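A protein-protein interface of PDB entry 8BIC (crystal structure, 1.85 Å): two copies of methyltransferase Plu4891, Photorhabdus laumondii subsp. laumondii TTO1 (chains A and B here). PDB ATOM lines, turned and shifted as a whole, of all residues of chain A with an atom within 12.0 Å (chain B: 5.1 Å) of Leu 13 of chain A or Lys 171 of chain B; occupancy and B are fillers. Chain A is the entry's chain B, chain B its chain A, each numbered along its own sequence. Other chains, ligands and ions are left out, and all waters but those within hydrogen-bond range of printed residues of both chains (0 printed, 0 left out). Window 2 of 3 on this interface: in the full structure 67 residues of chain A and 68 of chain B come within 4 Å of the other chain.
Of the 7 printed residues of chain A, 3 touch a printed residue of chain B. Hydrophobic or aromatic side chains of chain A that line the printed part of chain B: Leu 13 and Phe 15. Of the 12 printed residues of chain B, 4 touch a printed residue of chain A.
Leu 13 of chain A touches four residues of chain B. Lys 171 of chain B touches just one residue of chain A: Leu 13. No residue of chain A comes within 4 Å of Ile 168 of chain B. No residue of chain A comes within 4 Å of Glu 170 of chain B. No residue of chain A comes within 4 Å of Leu 172 of chain B. No residue of chain A comes within 4 Å of Ile 175 of chain B. Ile 323 of chain B touches just one residue of chain A: Leu 13. Glu 325 of chain B touches just these residues of chain A: Leu 13, Tyr 14 and Phe 15. Printed residues of chain B within 4 Å of Phe 15 of chain A: Glu 325 (2.9 Å). Of the printed residues of chain A, Asn 324 of chain B touches Leu 13 and Tyr 14. Printed residues of chain B within 4 Å of Tyr 14 of chain A: Asn 324 (3.99 Å) and Glu 325 (3.3 Å). Glu 322 of chain B touches none of the printed residues of chain A. Gly 17 of chain A touches none of the printed residues of chain B. The nearest printed residue of chain A that does not touch Asn 324 of chain B is Phe 15 of chain A (5.4 Å).
No position is printed for both chains.
Lys 171 of chain B touches Leu 13 of chain A. O of Ile 323 of chain B touches CD1 of Leu 13 of chain A, 3.4 Å away. CB of Leu 13 of chain A touches CA of Asn 324 of chain B (3.4 Å). N of Tyr 14 of chain A touches CB of Asn 324 of chain B (3.99 Å).
OE2 of Glu 325 of chain B is in hydrogen-bond range of N of Tyr 14 of chain A (3.3 Å). The backbone NH (N) of Phe 15 of chain A lies within hydrogen-bond range of the side-chain carboxylate (OE2) of Glu 325 of chain B, 2.9 Å away. N of Leu 13 of chain A sits close to N of Glu 325 of chain B.
The backbone carbonyl oxygen (O) of Glu 322 of chain B is in hydrogen-bond range of the side-chain amino group (NZ) of Lys 171 of chain B. The side-chain amino group of Lys 171 of chain B lies within hydrogen-bond range of the backbone carbonyl oxygen of Ile 323 of chain B, 3.1 Å away.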
ATOM      1  N   LEU A  13       5.205 -15.852 -14.513  1.00  0.00           N
ATOM      2  CA  LEU A  13       6.366 -16.789 -14.524  1.00  0.00           C
ATOM      3  C   LEU A  13       5.860 -18.238 -14.628  1.00  0.00           C
ATOM      4  O   LEU A  13       5.889 -18.788 -15.743  1.00  0.00           O
ATOM      5  CB  LEU A  13       7.203 -16.554 -13.260  1.00  0.00           C
ATOM      6  CG  LEU A  13       8.675 -16.949 -13.339  1.00  0.00           C
ATOM      7  CD1 LEU A  13       9.470 -16.231 -12.265  1.00  0.00           C
ATOM      8  CD2 LEU A  13       8.854 -18.458 -13.219  1.00  0.00           C
ATOM      9  N   TYR A  14       5.385 -18.815 -13.519  1.00  0.00           N
ATOM     10  CA  TYR A  14       5.086 -20.264 -13.355  1.00  0.00           C
ATOM     11  C   TYR A  14       3.826 -20.660 -14.139  1.00  0.00           C
ATOM     12  O   TYR A  14       3.951 -21.415 -15.120  1.00  0.00           O
ATOM     13  CB  TYR A  14       4.930 -20.617 -11.872  1.00  0.00           C
ATOM     14  CG  TYR A  14       6.169 -21.184 -11.230  1.00  0.00           C
ATOM     15  CD1 TYR A  14       6.603 -22.466 -11.535  1.00  0.00           C
ATOM     16  CD2 TYR A  14       6.908 -20.444 -10.320  1.00  0.00           C
ATOM     17  CE1 TYR A  14       7.741 -22.999 -10.951  1.00  0.00           C
ATOM     18  CE2 TYR A  14       8.049 -20.961  -9.729  1.00  0.00           C
ATOM     19  CZ  TYR A  14       8.467 -22.244 -10.045  1.00  0.00           C
ATOM     20  OH  TYR A  14       9.590 -22.763  -9.468  1.00  0.00           O
ATOM     21  N   PHE A  15       2.654 -20.187 -13.698  1.00  0.00           N
ATOM     22  CA  PHE A  15       1.301 -20.600 -14.170  1.00  0.00           C
ATOM     23  C   PHE A  15       1.011 -22.049 -13.748  1.00  0.00           C
ATOM     24  O   PHE A  15       0.317 -22.766 -14.492  1.00  0.00           O
ATOM     25  CB  PHE A  15       1.151 -20.428 -15.688  1.00  0.00           C
ATOM     26  CG  PHE A  15       0.857 -19.020 -16.136  1.00  0.00           C
ATOM     27  CD1 PHE A  15      -0.439 -18.621 -16.423  1.00  0.00           C
ATOM     28  CD2 PHE A  15       1.877 -18.092 -16.266  1.00  0.00           C
ATOM     29  CE1 PHE A  15      -0.708 -17.323 -16.829  1.00  0.00           C
ATOM     30  CE2 PHE A  15       1.604 -16.796 -16.672  1.00  0.00           C
ATOM     31  CZ  PHE A  15       0.316 -16.413 -16.958  1.00  0.00           C
ATOM     32  N   GLN A  16       1.501 -22.462 -12.573  1.00  0.00           N
ATOM     33  CA  GLN A  16       1.276 -23.825 -12.017  1.00  0.00           C
ATOM     34  C   GLN A  16      -0.202 -23.967 -11.646  1.00  0.00           C
ATOM     35  O   GLN A  16      -0.655 -23.221 -10.760  1.00  0.00           O
ATOM     36  CB  GLN A  16       2.145 -24.084 -10.783  1.00  0.00           C
ATOM     37  CG  GLN A  16       3.641 -24.047 -11.062  1.00  0.00           C
ATOM     38  CD  GLN A  16       4.096 -25.180 -11.946  1.00  0.00           C
ATOM     39  OE1 GLN A  16       4.510 -24.971 -13.085  1.00  0.00           O
ATOM     40  NE2 GLN A  16       4.009 -26.394 -11.425  1.00  0.00           N
ATOM     41  N   GLY A  17      -0.914 -24.872 -12.325  1.00  0.00           N
ATOM     42  CA  GLY A  17      -2.308 -25.248 -12.028  1.00  0.00           C
ATOM     43  C   GLY A  17      -3.315 -24.216 -12.511  1.00  0.00           C
ATOM     44  O   GLY A  17      -4.463 -24.282 -12.051  1.00  0.00           O
ATOM     45  N   SER A  18      -2.923 -23.320 -13.424  1.00  0.00           N
ATOM     46  CA  SER A  18      -3.753 -22.175 -13.889  1.00  0.00           C
ATOM     47  C   SER A  18      -5.032 -22.697 -14.564  1.00  0.00           C
ATOM     48  O   SER A  18      -6.106 -22.118 -14.327  1.00  0.00           O
ATOM     49  CB  SER A  18      -2.986 -21.247 -14.799  1.00  0.00           C
ATOM     50  OG  SER A  18      -2.859 -21.807 -16.100  1.00  0.00           O
ATOM     51  N   MET A  19      -4.942 -23.764 -15.361  1.00  0.00           N
ATOM     52  CA  MET A  19      -6.135 -24.333 -16.044  1.00  0.00           C
ATOM     53  C   MET A  19      -7.117 -24.889 -14.994  1.00  0.00           C
ATOM     54  O   MET A  19      -8.325 -24.562 -15.074  1.00  0.00           O
ATOM     55  CB  MET A  19      -5.727 -25.426 -17.034  1.00  0.00           C
ATOM     56  CG  MET A  19      -6.864 -25.904 -17.907  1.00  0.00           C
ATOM     57  SD  MET A  19      -7.797 -27.240 -17.134  1.00  0.00           S
ATOM     58  CE  MET A  19      -8.018 -28.316 -18.553  1.00  0.00           C
ATOM     59  N   ILE B 168       4.992 -21.104  -3.248  1.00  0.00           N
ATOM     60  CA  ILE B 168       5.896 -19.970  -3.616  1.00  0.00           C
ATOM     61  C   ILE B 168       7.155 -19.956  -2.741  1.00  0.00           C
ATOM     62  O   ILE B 168       8.016 -19.096  -3.002  1.00  0.00           O
ATOM     63  CB  ILE B 168       5.152 -18.620  -3.546  1.00  0.00           C
ATOM     64  CG1 ILE B 168       4.886 -18.173  -2.105  1.00  0.00           C
ATOM     65  CG2 ILE B 168       3.874 -18.670  -4.366  1.00  0.00           C
ATOM     66  CD1 ILE B 168       4.634 -16.687  -1.959  1.00  0.00           C
ATOM     67  N   ILE B 169       7.262 -20.844  -1.746  1.00  0.00           N
ATOM     68  CA  ILE B 169       8.317 -20.751  -0.693  1.00  0.00           C
ATOM     69  C   ILE B 169       9.700 -20.919  -1.329  1.00  0.00           C
ATOM     70  O   ILE B 169      10.622 -20.192  -0.919  1.00  0.00           O
ATOM     71  CB  ILE B 169       8.108 -21.748   0.465  1.00  0.00           C
ATOM     72  CG1 ILE B 169       9.119 -21.494   1.587  1.00  0.00           C
ATOM     73  CG2 ILE B 169       8.151 -23.196  -0.005  1.00  0.00           C
ATOM     74  CD1 ILE B 169       9.165 -20.059   2.077  1.00  0.00           C
ATOM     75  N   GLU B 170       9.841 -21.847  -2.275  1.00  0.00           N
ATOM     76  CA  GLU B 170      11.134 -22.121  -2.955  1.00  0.00           C
ATOM     77  C   GLU B 170      11.599 -20.818  -3.617  1.00  0.00           C
ATOM     78  O   GLU B 170      12.701 -20.341  -3.290  1.00  0.00           O
ATOM     79  CB  GLU B 170      10.980 -23.276  -3.950  1.00  0.00           C
ATOM     80  CG  GLU B 170      12.300 -23.813  -4.463  1.00  0.00           C
ATOM     81  CD  GLU B 170      12.167 -24.857  -5.560  1.00  0.00           C
ATOM     82  OE1 GLU B 170      12.668 -24.605  -6.673  1.00  0.00           O
ATOM     83  OE2 GLU B 170      11.564 -25.918  -5.296  1.00  0.00           O
ATOM     84  N   LYS B 171      10.753 -20.236  -4.467  1.00  0.00           N
ATOM     85  CA  LYS B 171      11.064 -19.005  -5.239  1.00  0.00           C
ATOM     86  C   LYS B 171      11.350 -17.846  -4.275  1.00  0.00           C
ATOM     87  O   LYS B 171      12.201 -16.992  -4.600  1.00  0.00           O
ATOM     88  CB  LYS B 171       9.908 -18.656  -6.180  1.00  0.00           C
ATOM     89  CG  LYS B 171      10.131 -17.429  -7.053  1.00  0.00           C
ATOM     90  CD  LYS B 171      11.439 -17.454  -7.823  1.00  0.00           C
ATOM     91  CE  LYS B 171      11.771 -16.111  -8.428  1.00  0.00           C
ATOM     92  NZ  LYS B 171      10.970 -15.854  -9.641  1.00  0.00           N
ATOM     93  N   LEU B 172      10.663 -17.823  -3.132  1.00  0.00           N
ATOM     94  CA  LEU B 172      10.748 -16.730  -2.129  1.00  0.00           C
ATOM     95  C   LEU B 172      12.143 -16.686  -1.495  1.00  0.00           C
ATOM     96  O   LEU B 172      12.697 -15.577  -1.369  1.00  0.00           O
ATOM     97  CB  LEU B 172       9.672 -16.956  -1.065  1.00  0.00           C
ATOM     98  CG  LEU B 172       9.420 -15.770  -0.143  1.00  0.00           C
ATOM     99  CD1 LEU B 172       9.134 -14.521  -0.954  1.00  0.00           C
ATOM    100  CD2 LEU B 172       8.273 -16.061   0.815  1.00  0.00           C
ATOM    101  N   LEU B 173      12.675 -17.848  -1.101  1.00  0.00           N
ATOM    102  CA  LEU B 173      13.987 -17.995  -0.412  1.00  0.00           C
ATOM    103  C   LEU B 173      15.131 -17.613  -1.362  1.00  0.00           C
ATOM    104  O   LEU B 173      16.174 -17.155  -0.865  1.00  0.00           O
ATOM    105  CB  LEU B 173      14.134 -19.437   0.080  1.00  0.00           C
ATOM    106  CG  LEU B 173      13.151 -19.858   1.172  1.00  0.00           C
ATOM    107  CD1 LEU B 173      13.097 -21.372   1.309  1.00  0.00           C
ATOM    108  CD2 LEU B 173      13.509 -19.215   2.500  1.00  0.00           C
ATOM    109  N   ASP B 174      14.935 -17.788  -2.672  1.00  0.00           N
ATOM    110  CA  ASP B 174      15.941 -17.469  -3.721  1.00  0.00           C
ATOM    111  C   ASP B 174      16.110 -15.950  -3.846  1.00  0.00           C
ATOM    112  O   ASP B 174      17.258 -15.486  -3.799  1.00  0.00           O
ATOM    113  CB  ASP B 174      15.551 -18.071  -5.074  1.00  0.00           C
ATOM    114  CG  ASP B 174      16.174 -19.428  -5.340  1.00  0.00           C
ATOM    115  OD1 ASP B 174      16.382 -20.182  -4.369  1.00  0.00           O
ATOM    116  OD2 ASP B 174      16.463 -19.709  -6.515  1.00  0.00           O
ATOM    117  N   ILE B 175      15.007 -15.213  -3.997  1.00  0.00           N
ATOM    118  CA  ILE B 175      15.014 -13.784  -4.442  1.00  0.00           C
ATOM    119  C   ILE B 175      15.158 -12.835  -3.249  1.00  0.00           C
ATOM    120  O   ILE B 175      15.417 -11.641  -3.495  1.00  0.00           O
ATOM    121  CB  ILE B 175      13.757 -13.451  -5.269  1.00  0.00           C
ATOM    122  CG1 ILE B 175      12.479 -13.506  -4.424  1.00  0.00           C
ATOM    123  CG2 ILE B 175      13.693 -14.342  -6.499  1.00  0.00           C
ATOM    124  CD1 ILE B 175      11.205 -13.613  -5.225  1.00  0.00           C
ATOM    125  N   GLU B 322       9.550  -9.938  -8.594  1.00  0.00           N
ATOM    126  CA  GLU B 322       8.500 -10.849  -9.115  1.00  0.00           C
ATOM    127  C   GLU B 322       8.746 -12.252  -8.550  1.00  0.00           C
ATOM    128  O   GLU B 322       9.886 -12.728  -8.620  1.00  0.00           O
ATOM    129  CB  GLU B 322       8.508 -10.859 -10.646  1.00  0.00           C
ATOM    130  CG  GLU B 322       8.197  -9.506 -11.267  1.00  0.00           C
ATOM    131  CD  GLU B 322       6.783  -9.014 -11.009  1.00  0.00           C
ATOM    132  OE1 GLU B 322       5.834  -9.738 -11.380  1.00  0.00           O
ATOM    133  OE2 GLU B 322       6.632  -7.919 -10.419  1.00  0.00           O
ATOM    134  N   ILE B 323       7.715 -12.875  -7.980  1.00  0.00           N
ATOM    135  CA  ILE B 323       7.732 -14.314  -7.591  1.00  0.00           C
ATOM    136  C   ILE B 323       7.246 -15.119  -8.798  1.00  0.00           C
ATOM    137  O   ILE B 323       7.949 -16.054  -9.206  1.00  0.00           O
ATOM    138  CB  ILE B 323       6.879 -14.572  -6.335  1.00  0.00           C
ATOM    139  CG1 ILE B 323       7.405 -13.790  -5.128  1.00  0.00           C
ATOM    140  CG2 ILE B 323       6.787 -16.064  -6.049  1.00  0.00           C
ATOM    141  CD1 ILE B 323       6.500 -13.835  -3.915  1.00  0.00           C
ATOM    142  N   ASN B 324       6.086 -14.749  -9.342  1.00  0.00           N
ATOM    143  CA  ASN B 324       5.477 -15.408 -10.524  1.00  0.00           C
ATOM    144  C   ASN B 324       4.501 -14.426 -11.187  1.00  0.00           C
ATOM    145  O   ASN B 324       4.634 -13.213 -10.940  1.00  0.00           O
ATOM    146  CB  ASN B 324       4.875 -16.761 -10.134  1.00  0.00           C
ATOM    147  CG  ASN B 324       3.794 -16.672  -9.075  1.00  0.00           C
ATOM    148  OD1 ASN B 324       3.115 -15.655  -8.936  1.00  0.00           O
ATOM    149  ND2 ASN B 324       3.624 -17.746  -8.325  1.00  0.00           N
ATOM    150  N   GLU B 325       3.576 -14.934 -12.011  1.00  0.00           N
ATOM    151  CA  GLU B 325       2.611 -14.129 -12.810  1.00  0.00           C
ATOM    152  C   GLU B 325       1.586 -13.468 -11.880  1.00  0.00           C
ATOM    153  O   GLU B 325       1.045 -12.413 -12.260  1.00  0.00           O
ATOM    154  CB  GLU B 325       1.926 -14.995 -13.875  1.00  0.00           C
ATOM    155  CG  GLU B 325       0.822 -15.912 -13.359  1.00  0.00           C
ATOM    156  CD  GLU B 325       1.251 -17.212 -12.694  1.00  0.00           C
ATOM    157  OE1 GLU B 325       0.359 -17.976 -12.267  1.00  0.00           O
ATOM    158  OE2 GLU B 325       2.472 -17.469 -12.609  1.00  0.00           O
